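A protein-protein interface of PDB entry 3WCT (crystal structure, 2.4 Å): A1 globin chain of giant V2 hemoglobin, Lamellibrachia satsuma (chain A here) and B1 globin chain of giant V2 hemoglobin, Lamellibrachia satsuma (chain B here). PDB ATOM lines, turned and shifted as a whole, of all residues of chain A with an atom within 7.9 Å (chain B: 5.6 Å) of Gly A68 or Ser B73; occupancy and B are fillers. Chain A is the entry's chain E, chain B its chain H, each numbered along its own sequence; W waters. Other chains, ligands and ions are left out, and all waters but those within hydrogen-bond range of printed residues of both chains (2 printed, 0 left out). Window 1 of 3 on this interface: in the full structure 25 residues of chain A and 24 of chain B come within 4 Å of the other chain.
CA of Arg A65 touches SD of Met B77, 3.7 Å away.
Arg A72 touches Val B69 (CB to CG1, 3.5 Å).
Arg B70 touches Arg A72.
Met A76 touches Val B69 (CE to CG1, 3.9 Å).
Of the 21 printed residues of chain A, 7 touch a printed residue of chain B.
Hydrophobic or aromatic side chains of chain A that line the printed part of chain B: Ala A64 and Met A76.
Among the printed residues, 8 pairs touch across the chains.
Among the printed residues, Asp or Glu carboxylates within 4 Å of a Lys or Arg side-chain nitrogen of the other chain: Arg A24 with Asp B76 and Asp A86 with Arg B70.
Of chain B, only Ser B73 comes within 4 Å of Gly A68.
Printed residues of chain B within 4 Å of Met A76: Val B69.
Printed residues of chain A within 4 Å of Val B69: Arg A72 (3.5 Å) and Met A76 (3.9 Å).
Of chain A, only Gly A68 comes within 4 Å of Ser B73.
No residue of chain A comes within 4 Å of Gly B74.
Of the printed residues of chain A, Asp B76 touches Arg A24 (3.1 Å).
The nearest printed residue of chain A that does not touch Asp B76 is Tyr A18 (4.9 Å).
Water W1 lies within hydrogen-bond range of OH of Tyr B20 (2.8 Å), OD2 of Asp A71 (3.0 Å) and OG of Ser B73 (3.1 Å).
Water W2 lies within hydrogen-bond range of the side-chain hydroxyl of Tyr A18 (3.0 Å), the side-chain carboxylate of Asp B76 (3.0 Å) and the side-chain carboxylate of Asp A71 (3.3 Å).
The guanidinium group (NH1) of Arg A65 sits close to the backbone carbonyl oxygen (O) of Ala A61 (3.5 Å).
The backbone carbonyl oxygen of Arg A72 lies within hydrogen-bond range of the side-chain hydroxyl of Ser A75 (2.8 Å).
The guanidinium group of Arg A72 is in salt-bridge range of the side-chain carboxylate of Asp A86.
NH1 of Arg A24 lies within salt-bridge range of OD1 of Asp B76.
The backbone carbonyl oxygen (O) of Gly A68 sits at hydrogen-bond distance from the side-chain hydroxyl (OG) of Ser B73 (3.5 Å).
The side-chain carboxylate (OD1) of Asp A86 lies within salt-bridge range of the guanidinium group (NE) of Arg B70, 3.0 Å away.
O of Ala A64 sits close to SD of Met B77, at 3.6 Å.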
ATOM      1  N   TRP A  14       6.399  22.593  -9.371  1.00  0.00           N
ATOM      2  CA  TRP A  14       6.182  22.758 -10.804  1.00  0.00           C
ATOM      3  C   TRP A  14       7.208  23.768 -11.337  1.00  0.00           C
ATOM      4  O   TRP A  14       7.990  23.455 -12.237  1.00  0.00           O
ATOM      5  CB  TRP A  14       4.755  23.252 -11.081  1.00  0.00           C
ATOM      6  CG  TRP A  14       4.553  23.851 -12.447  1.00  0.00           C
ATOM      7  CD1 TRP A  14       4.564  25.177 -12.773  1.00  0.00           C
ATOM      8  CD2 TRP A  14       4.334  23.141 -13.676  1.00  0.00           C
ATOM      9  NE1 TRP A  14       4.370  25.341 -14.132  1.00  0.00           N
ATOM     10  CE2 TRP A  14       4.227  24.104 -14.708  1.00  0.00           C
ATOM     11  CE3 TRP A  14       4.226  21.784 -14.005  1.00  0.00           C
ATOM     12  CZ2 TRP A  14       4.009  23.751 -16.044  1.00  0.00           C
ATOM     13  CZ3 TRP A  14       4.010  21.432 -15.333  1.00  0.00           C
ATOM     14  CH2 TRP A  14       3.905  22.414 -16.337  1.00  0.00           C
ATOM     15  N   TYR A  18       9.474  22.736 -14.390  1.00  0.00           N
ATOM     16  CA  TYR A  18       9.081  23.311 -15.681  1.00  0.00           C
ATOM     17  C   TYR A  18      10.201  24.098 -16.361  1.00  0.00           C
ATOM     18  O   TYR A  18      10.354  24.042 -17.582  1.00  0.00           O
ATOM     19  CB  TYR A  18       7.846  24.203 -15.496  1.00  0.00           C
ATOM     20  CG  TYR A  18       7.263  24.762 -16.777  1.00  0.00           C
ATOM     21  CD1 TYR A  18       6.962  23.934 -17.853  1.00  0.00           C
ATOM     22  CD2 TYR A  18       6.977  26.111 -16.892  1.00  0.00           C
ATOM     23  CE1 TYR A  18       6.385  24.441 -19.019  1.00  0.00           C
ATOM     24  CE2 TYR A  18       6.404  26.630 -18.045  1.00  0.00           C
ATOM     25  CZ  TYR A  18       6.107  25.788 -19.106  1.00  0.00           C
ATOM     26  OH  TYR A  18       5.504  26.307 -20.231  1.00  0.00           O
ATOM     27  N   ARG A  24      11.375  23.761 -21.450  1.00  0.00           N
ATOM     28  CA  ARG A  24       9.934  23.564 -21.395  1.00  0.00           C
ATOM     29  C   ARG A  24       9.484  22.629 -22.506  1.00  0.00           C
ATOM     30  O   ARG A  24       8.663  21.743 -22.285  1.00  0.00           O
ATOM     31  CB  ARG A  24       9.213  24.898 -21.532  1.00  0.00           C
ATOM     32  CG  ARG A  24       9.551  25.907 -20.453  1.00  0.00           C
ATOM     33  CD  ARG A  24       8.835  27.202 -20.759  1.00  0.00           C
ATOM     34  NE  ARG A  24       9.200  28.296 -19.871  1.00  0.00           N
ATOM     35  CZ  ARG A  24       8.778  29.542 -20.046  1.00  0.00           C
ATOM     36  NH1 ARG A  24       7.982  29.825 -21.070  1.00  0.00           N
ATOM     37  NH2 ARG A  24       9.156  30.501 -19.212  1.00  0.00           N
ATOM     38  N   ALA A  61       3.006  22.220 -31.330  1.00  0.00           N
ATOM     39  CA  ALA A  61       2.202  23.386 -30.995  1.00  0.00           C
ATOM     40  C   ALA A  61       1.205  22.919 -29.947  1.00  0.00           C
ATOM     41  O   ALA A  61       0.867  23.657 -29.015  1.00  0.00           O
ATOM     42  CB  ALA A  61       1.463  23.895 -32.229  1.00  0.00           C
ATOM     43  N   HIS A  62       0.739  21.680 -30.107  1.00  0.00           N
ATOM     44  CA  HIS A  62      -0.211  21.109 -29.172  1.00  0.00           C
ATOM     45  C   HIS A  62       0.448  20.817 -27.820  1.00  0.00           C
ATOM     46  O   HIS A  62      -0.184  20.944 -26.775  1.00  0.00           O
ATOM     47  CB  HIS A  62      -0.820  19.823 -29.720  1.00  0.00           C
ATOM     48  CG  HIS A  62      -1.634  19.087 -28.705  1.00  0.00           C
ATOM     49  ND1 HIS A  62      -2.810  19.594 -28.198  1.00  0.00           N
ATOM     50  CD2 HIS A  62      -1.375  17.959 -28.002  1.00  0.00           C
ATOM     51  CE1 HIS A  62      -3.240  18.812 -27.223  1.00  0.00           C
ATOM     52  NE2 HIS A  62      -2.385  17.813 -27.084  1.00  0.00           N
ATOM     53  N   ILE A  63       1.708  20.404 -27.842  1.00  0.00           N
ATOM     54  CA  ILE A  63       2.419  20.132 -26.606  1.00  0.00           C
ATOM     55  C   ILE A  63       2.563  21.430 -25.811  1.00  0.00           C
ATOM     56  O   ILE A  63       2.334  21.456 -24.601  1.00  0.00           O
ATOM     57  CB  ILE A  63       3.814  19.539 -26.886  1.00  0.00           C
ATOM     58  CG1 ILE A  63       3.665  18.100 -27.398  1.00  0.00           C
ATOM     59  CG2 ILE A  63       4.683  19.621 -25.629  1.00  0.00           C
ATOM     60  CD1 ILE A  63       4.986  17.346 -27.569  1.00  0.00           C
ATOM     61  N   ALA A  64       2.920  22.509 -26.503  1.00  0.00           N
ATOM     62  CA  ALA A  64       3.087  23.814 -25.867  1.00  0.00           C
ATOM     63  C   ALA A  64       1.783  24.380 -25.303  1.00  0.00           C
ATOM     64  O   ALA A  64       1.782  25.007 -24.244  1.00  0.00           O
ATOM     65  CB  ALA A  64       3.700  24.810 -26.859  1.00  0.00           C
ATOM     66  N   ARG A  65       0.675  24.178 -26.003  1.00  0.00           N
ATOM     67  CA  ARG A  65      -0.599  24.688 -25.504  1.00  0.00           C
ATOM     68  C   ARG A  65      -0.975  23.994 -24.204  1.00  0.00           C
ATOM     69  O   ARG A  65      -1.432  24.635 -23.259  1.00  0.00           O
ATOM     70  CB  ARG A  65      -1.706  24.486 -26.536  1.00  0.00           C
ATOM     71  CG  ARG A  65      -1.748  25.570 -27.588  1.00  0.00           C
ATOM     72  CD  ARG A  65      -2.962  25.405 -28.501  1.00  0.00           C
ATOM     73  NE  ARG A  65      -2.853  24.226 -29.347  1.00  0.00           N
ATOM     74  CZ  ARG A  65      -2.182  24.185 -30.497  1.00  0.00           C
ATOM     75  NH1 ARG A  65      -1.554  25.268 -30.943  1.00  0.00           N
ATOM     76  NH2 ARG A  65      -2.150  23.062 -31.210  1.00  0.00           N
ATOM     77  N   VAL A  66      -0.761  22.682 -24.166  1.00  0.00           N
ATOM     78  CA  VAL A  66      -1.076  21.869 -22.992  1.00  0.00           C
ATOM     79  C   VAL A  66      -0.242  22.243 -21.756  1.00  0.00           C
ATOM     80  O   VAL A  66      -0.797  22.548 -20.700  1.00  0.00           O
ATOM     81  CB  VAL A  66      -0.898  20.350 -23.310  1.00  0.00           C
ATOM     82  CG1 VAL A  66      -1.011  19.519 -22.038  1.00  0.00           C
ATOM     83  CG2 VAL A  66      -1.962  19.903 -24.315  1.00  0.00           C
ATOM     84  N   ILE A  67       1.082  22.226 -21.865  1.00  0.00           N
ATOM     85  CA  ILE A  67       1.880  22.585 -20.705  1.00  0.00           C
ATOM     86  C   ILE A  67       1.615  24.050 -20.374  1.00  0.00           C
ATOM     87  O   ILE A  67       1.744  24.469 -19.228  1.00  0.00           O
ATOM     88  CB  ILE A  67       3.389  22.355 -20.943  1.00  0.00           C
ATOM     89  CG1 ILE A  67       3.833  23.065 -22.219  1.00  0.00           C
ATOM     90  CG2 ILE A  67       3.679  20.861 -21.012  1.00  0.00           C
ATOM     91  CD1 ILE A  67       5.329  22.996 -22.473  1.00  0.00           C
ATOM     92  N   GLY A  68       1.229  24.823 -21.383  1.00  0.00           N
ATOM     93  CA  GLY A  68       0.928  26.218 -21.148  1.00  0.00           C
ATOM     94  C   GLY A  68      -0.322  26.302 -20.295  1.00  0.00           C
ATOM     95  O   GLY A  68      -0.481  27.216 -19.479  1.00  0.00           O
ATOM     96  N   GLY A  69      -1.221  25.344 -20.491  1.00  0.00           N
ATOM     97  CA  GLY A  69      -2.441  25.313 -19.710  1.00  0.00           C
ATOM     98  C   GLY A  69      -2.097  24.886 -18.299  1.00  0.00           C
ATOM     99  O   GLY A  69      -2.548  25.484 -17.318  1.00  0.00           O
ATOM    100  N   LEU A  70      -1.291  23.840 -18.195  1.00  0.00           N
ATOM    101  CA  LEU A  70      -0.872  23.355 -16.893  1.00  0.00           C
ATOM    102  C   LEU A  70      -0.276  24.507 -16.097  1.00  0.00           C
ATOM    103  O   LEU A  70      -0.628  24.713 -14.938  1.00  0.00           O
ATOM    104  CB  LEU A  70       0.168  22.243 -17.050  1.00  0.00           C
ATOM    105  CG  LEU A  70      -0.376  20.896 -17.498  1.00  0.00           C
ATOM    106  CD1 LEU A  70       0.761  20.006 -17.997  1.00  0.00           C
ATOM    107  CD2 LEU A  70      -1.126  20.250 -16.339  1.00  0.00           C
ATOM    108  N   ASP A  71       0.612  25.266 -16.737  1.00  0.00           N
ATOM    109  CA  ASP A  71       1.280  26.395 -16.086  1.00  0.00           C
ATOM    110  C   ASP A  71       0.322  27.448 -15.534  1.00  0.00           C
ATOM    111  O   ASP A  71       0.366  27.771 -14.348  1.00  0.00           O
ATOM    112  CB  ASP A  71       2.251  27.087 -17.051  1.00  0.00           C
ATOM    113  CG  ASP A  71       3.113  28.129 -16.356  1.00  0.00           C
ATOM    114  OD1 ASP A  71       3.986  27.746 -15.554  1.00  0.00           O
ATOM    115  OD2 ASP A  71       2.912  29.328 -16.606  1.00  0.00           O
ATOM    116  N   ARG A  72      -0.524  28.000 -16.398  1.00  0.00           N
ATOM    117  CA  ARG A  72      -1.465  29.025 -15.959  1.00  0.00           C
ATOM    118  C   ARG A  72      -2.413  28.449 -14.908  1.00  0.00           C
ATOM    119  O   ARG A  72      -2.725  29.106 -13.919  1.00  0.00           O
ATOM    120  CB  ARG A  72      -2.247  29.583 -17.155  1.00  0.00           C
ATOM    121  CG  ARG A  72      -3.128  28.569 -17.865  1.00  0.00           C
ATOM    122  CD  ARG A  72      -3.736  29.148 -19.145  1.00  0.00           C
ATOM    123  NE  ARG A  72      -5.113  28.685 -19.308  1.00  0.00           N
ATOM    124  CZ  ARG A  72      -5.632  28.182 -20.424  1.00  0.00           C
ATOM    125  NH1 ARG A  72      -4.902  28.063 -21.529  1.00  0.00           N
ATOM    126  NH2 ARG A  72      -6.893  27.776 -20.421  1.00  0.00           N
ATOM    127  N   VAL A  73      -2.837  27.204 -15.103  1.00  0.00           N
ATOM    128  CA  VAL A  73      -3.743  26.567 -14.154  1.00  0.00           C
ATOM    129  C   VAL A  73      -3.075  26.396 -12.791  1.00  0.00           C
ATOM    130  O   VAL A  73      -3.682  26.673 -11.750  1.00  0.00           O
ATOM    131  CB  VAL A  73      -4.217  25.195 -14.681  1.00  0.00           C
ATOM    132  CG1 VAL A  73      -4.960  24.437 -13.591  1.00  0.00           C
ATOM    133  CG2 VAL A  73      -5.119  25.398 -15.890  1.00  0.00           C
ATOM    134  N   ILE A  74      -1.823  25.953 -12.796  1.00  0.00           N
ATOM    135  CA  ILE A  74      -1.093  25.761 -11.554  1.00  0.00           C
ATOM    136  C   ILE A  74      -0.785  27.099 -10.865  1.00  0.00           C
ATOM    137  O   ILE A  74      -0.744  27.176  -9.632  1.00  0.00           O
ATOM    138  CB  ILE A  74       0.212  24.953 -11.811  1.00  0.00           C
ATOM    139  CG1 ILE A  74      -0.117  23.456 -11.872  1.00  0.00           C
ATOM    140  CG2 ILE A  74       1.238  25.236 -10.727  1.00  0.00           C
ATOM    141  CD1 ILE A  74       1.055  22.567 -12.285  1.00  0.00           C
ATOM    142  N   SER A  75      -0.596  28.150 -11.660  1.00  0.00           N
ATOM    143  CA  SER A  75      -0.296  29.469 -11.118  1.00  0.00           C
ATOM    144  C   SER A  75      -1.515  30.104 -10.456  1.00  0.00           C
ATOM    145  O   SER A  75      -1.377  31.029  -9.652  1.00  0.00           O
ATOM    146  CB  SER A  75       0.217  30.399 -12.217  1.00  0.00           C
ATOM    147  OG  SER A  75      -0.854  30.904 -12.995  1.00  0.00           O
ATOM    148  N   MET A  76      -2.706  29.615 -10.794  1.00  0.00           N
ATOM    149  CA  MET A  76      -3.935  30.155 -10.220  1.00  0.00           C
ATOM    150  C   MET A  76      -4.420  29.305  -9.053  1.00  0.00           C
ATOM    151  O   MET A  76      -5.456  29.601  -8.463  1.00  0.00           O
ATOM    152  CB  MET A  76      -5.042  30.240 -11.283  1.00  0.00           C
ATOM    153  CG  MET A  76      -4.840  31.320 -12.357  1.00  0.00           C
ATOM    154  SD  MET A  76      -6.183  31.355 -13.619  1.00  0.00           S
ATOM    155  CE  MET A  76      -5.665  29.997 -14.712  1.00  0.00           C
ATOM    156  N   ASP A  86     -11.055  29.231 -15.404  1.00  0.00           N
ATOM    157  CA  ASP A  86     -10.194  28.663 -16.434  1.00  0.00           C
ATOM    158  C   ASP A  86     -10.404  27.165 -16.610  1.00  0.00           C
ATOM    159  O   ASP A  86     -10.303  26.653 -17.721  1.00  0.00           O
ATOM    160  CB  ASP A  86      -8.726  28.973 -16.128  1.00  0.00           C
ATOM    161  CG  ASP A  86      -7.854  28.928 -17.367  1.00  0.00           C
ATOM    162  OD1 ASP A  86      -8.311  29.378 -18.440  1.00  0.00           O
ATOM    163  OD2 ASP A  86      -6.705  28.453 -17.268  1.00  0.00           O
ATOM    164  N   LEU A  90     -11.540  25.230 -19.993  1.00  0.00           N
ATOM    165  CA  LEU A  90     -10.882  24.056 -20.541  1.00  0.00           C
ATOM    166  C   LEU A  90     -11.860  22.913 -20.758  1.00  0.00           C
ATOM    167  O   LEU A  90     -11.752  22.170 -21.739  1.00  0.00           O
ATOM    168  CB  LEU A  90      -9.754  23.610 -19.617  1.00  0.00           C
ATOM    169  CG  LEU A  90      -8.535  24.530 -19.619  1.00  0.00           C
ATOM    170  CD1 LEU A  90      -7.718  24.286 -18.363  1.00  0.00           C
ATOM    171  CD2 LEU A  90      -7.716  24.289 -20.877  1.00  0.00           C
ATOM    172  N   TYR B  20       7.829  36.998 -16.525  1.00  0.00           N
ATOM    173  CA  TYR B  20       6.885  35.906 -16.719  1.00  0.00           C
ATOM    174  C   TYR B  20       7.574  34.553 -16.759  1.00  0.00           C
ATOM    175  O   TYR B  20       8.460  34.319 -17.582  1.00  0.00           O
ATOM    176  CB  TYR B  20       6.122  36.115 -18.027  1.00  0.00           C
ATOM    177  CG  TYR B  20       4.951  35.179 -18.226  1.00  0.00           C
ATOM    178  CD1 TYR B  20       5.141  33.810 -18.432  1.00  0.00           C
ATOM    179  CD2 TYR B  20       3.642  35.669 -18.218  1.00  0.00           C
ATOM    180  CE1 TYR B  20       4.058  32.959 -18.622  1.00  0.00           C
ATOM    181  CE2 TYR B  20       2.555  34.829 -18.408  1.00  0.00           C
ATOM    182  CZ  TYR B  20       2.766  33.482 -18.610  1.00  0.00           C
ATOM    183  OH  TYR B  20       1.681  32.662 -18.817  1.00  0.00           O
ATOM    184  N   THR B  68      -7.250  37.174 -18.958  1.00  0.00           N
ATOM    185  CA  THR B  68      -5.945  37.806 -19.145  1.00  0.00           C
ATOM    186  C   THR B  68      -4.800  36.808 -18.943  1.00  0.00           C
ATOM    187  O   THR B  68      -3.771  36.886 -19.614  1.00  0.00           O
ATOM    188  CB  THR B  68      -5.743  38.981 -18.182  1.00  0.00           C
ATOM    189  OG1 THR B  68      -5.978  38.541 -16.841  1.00  0.00           O
ATOM    190  CG2 THR B  68      -6.687  40.122 -18.529  1.00  0.00           C
ATOM    191  N   VAL B  69      -4.992  35.862 -18.030  1.00  0.00           N
ATOM    192  CA  VAL B  69      -3.972  34.870 -17.756  1.00  0.00           C
ATOM    193  C   VAL B  69      -3.729  34.008 -18.984  1.00  0.00           C
ATOM    194  O   VAL B  69      -2.578  33.824 -19.386  1.00  0.00           O
ATOM    195  CB  VAL B  69      -4.352  33.997 -16.524  1.00  0.00           C
ATOM    196  CG1 VAL B  69      -3.475  32.748 -16.450  1.00  0.00           C
ATOM    197  CG2 VAL B  69      -4.169  34.811 -15.254  1.00  0.00           C
ATOM    198  N   ARG B  70      -4.792  33.502 -19.607  1.00  0.00           N
ATOM    199  CA  ARG B  70      -4.597  32.685 -20.798  1.00  0.00           C
ATOM    200  C   ARG B  70      -4.065  33.532 -21.955  1.00  0.00           C
ATOM    201  O   ARG B  70      -3.333  33.033 -22.799  1.00  0.00           O
ATOM    202  CB  ARG B  70      -5.880  31.916 -21.187  1.00  0.00           C
ATOM    203  CG  ARG B  70      -7.109  32.720 -21.569  1.00  0.00           C
ATOM    204  CD  ARG B  70      -8.298  31.771 -21.882  1.00  0.00           C
ATOM    205  NE  ARG B  70      -8.959  31.254 -20.684  1.00  0.00           N
ATOM    206  CZ  ARG B  70     -10.055  31.785 -20.141  1.00  0.00           C
ATOM    207  NH1 ARG B  70     -10.627  32.847 -20.693  1.00  0.00           N
ATOM    208  NH2 ARG B  70     -10.570  31.270 -19.032  1.00  0.00           N
ATOM    209  N   VAL B  71      -4.412  34.818 -21.978  1.00  0.00           N
ATOM    210  CA  VAL B  71      -3.906  35.725 -23.008  1.00  0.00           C
ATOM    211  C   VAL B  71      -2.379  35.774 -22.866  1.00  0.00           C
ATOM    212  O   VAL B  71      -1.637  35.357 -23.759  1.00  0.00           O
ATOM    213  CB  VAL B  71      -4.456  37.154 -22.822  1.00  0.00           C
ATOM    214  CG1 VAL B  71      -3.628  38.148 -23.619  1.00  0.00           C
ATOM    215  CG2 VAL B  71      -5.907  37.218 -23.272  1.00  0.00           C
ATOM    216  N   LEU B  72      -1.919  36.277 -21.729  1.00  0.00           N
ATOM    217  CA  LEU B  72      -0.490  36.368 -21.448  1.00  0.00           C
ATOM    218  C   LEU B  72       0.227  35.018 -21.644  1.00  0.00           C
ATOM    219  O   LEU B  72       1.378  34.976 -22.081  1.00  0.00           O
ATOM    220  CB  LEU B  72      -0.286  36.872 -20.020  1.00  0.00           C
ATOM    221  CG  LEU B  72      -0.790  38.299 -19.785  1.00  0.00           C
ATOM    222  CD1 LEU B  72      -0.648  38.648 -18.312  1.00  0.00           C
ATOM    223  CD2 LEU B  72      -0.006  39.275 -20.648  1.00  0.00           C
ATOM    224  N   SER B  73      -0.463  33.926 -21.323  1.00  0.00           N
ATOM    225  CA  SER B  73       0.086  32.586 -21.488  1.00  0.00           C
ATOM    226  C   SER B  73       0.243  32.339 -22.990  1.00  0.00           C
ATOM    227  O   SER B  73       1.176  31.648 -23.437  1.00  0.00           O
ATOM    228  CB  SER B  73      -0.865  31.549 -20.904  1.00  0.00           C
ATOM    229  OG  SER B  73      -0.375  30.244 -21.142  1.00  0.00           O
ATOM    230  N   GLY B  74      -0.679  32.912 -23.760  1.00  0.00           N
ATOM    231  CA  GLY B  74      -0.631  32.764 -25.203  1.00  0.00           C
ATOM    232  C   GLY B  74       0.513  33.574 -25.788  1.00  0.00           C
ATOM    233  O   GLY B  74       1.121  33.176 -26.783  1.00  0.00           O
ATOM    234  N   LEU B  75       0.800  34.715 -25.168  1.00  0.00           N
ATOM    235  CA  LEU B  75       1.873  35.588 -25.614  1.00  0.00           C
ATOM    236  C   LEU B  75       3.226  34.957 -25.237  1.00  0.00           C
ATOM    237  O   LEU B  75       4.215  35.049 -25.980  1.00  0.00           O
ATOM    238  CB  LEU B  75       1.714  36.963 -24.955  1.00  0.00           C
ATOM    239  CG  LEU B  75       2.770  38.041 -25.231  1.00  0.00           C
ATOM    240  CD1 LEU B  75       3.080  38.114 -26.713  1.00  0.00           C
ATOM    241  CD2 LEU B  75       2.259  39.380 -24.724  1.00  0.00           C
ATOM    242  N   ASP B  76       3.239  34.315 -24.073  1.00  0.00           N
ATOM    243  CA  ASP B  76       4.413  33.641 -23.541  1.00  0.00           C
ATOM    244  C   ASP B  76       4.853  32.508 -24.461  1.00  0.00           C
ATOM    245  O   ASP B  76       6.035  32.351 -24.803  1.00  0.00           O
ATOM    246  CB  ASP B  76       4.081  33.065 -22.170  1.00  0.00           C
ATOM    247  CG  ASP B  76       5.220  32.297 -21.589  1.00  0.00           C
ATOM    248  OD1 ASP B  76       5.147  31.046 -21.555  1.00  0.00           O
ATOM    249  OD2 ASP B  76       6.198  32.952 -21.174  1.00  0.00           O
ATOM    250  N   MET B  77       3.867  31.717 -24.841  1.00  0.00           N
ATOM    251  CA  MET B  77       4.046  30.582 -25.719  1.00  0.00           C
ATOM    252  C   MET B  77       4.657  31.100 -27.028  1.00  0.00           C
ATOM    253  O   MET B  77       5.648  30.560 -27.524  1.00  0.00           O
ATOM    254  CB  MET B  77       2.672  29.969 -25.960  1.00  0.00           C
ATOM    255  CG  MET B  77       2.627  28.491 -26.188  1.00  0.00           C
ATOM    256  SD  MET B  77       0.895  27.987 -26.076  1.00  0.00           S
ATOM    257  CE  MET B  77       0.163  28.963 -27.408  1.00  0.00           C
ATOM    258  N   GLY B  78       4.074  32.168 -27.563  1.00  0.00           N
ATOM    259  CA  GLY B  78       4.562  32.741 -28.803  1.00  0.00           C
ATOM    260  C   GLY B  78       5.993  33.239 -28.726  1.00  0.00           C
ATOM    261  O   GLY B  78       6.796  32.999 -29.626  1.00  0.00           O
HETATM  262  O   HOH W   1       2.181  30.015 -19.393  1.00  0.00           O
HETATM  263  O   HOH W   2       4.858  29.061 -19.303  1.00  0.00           O
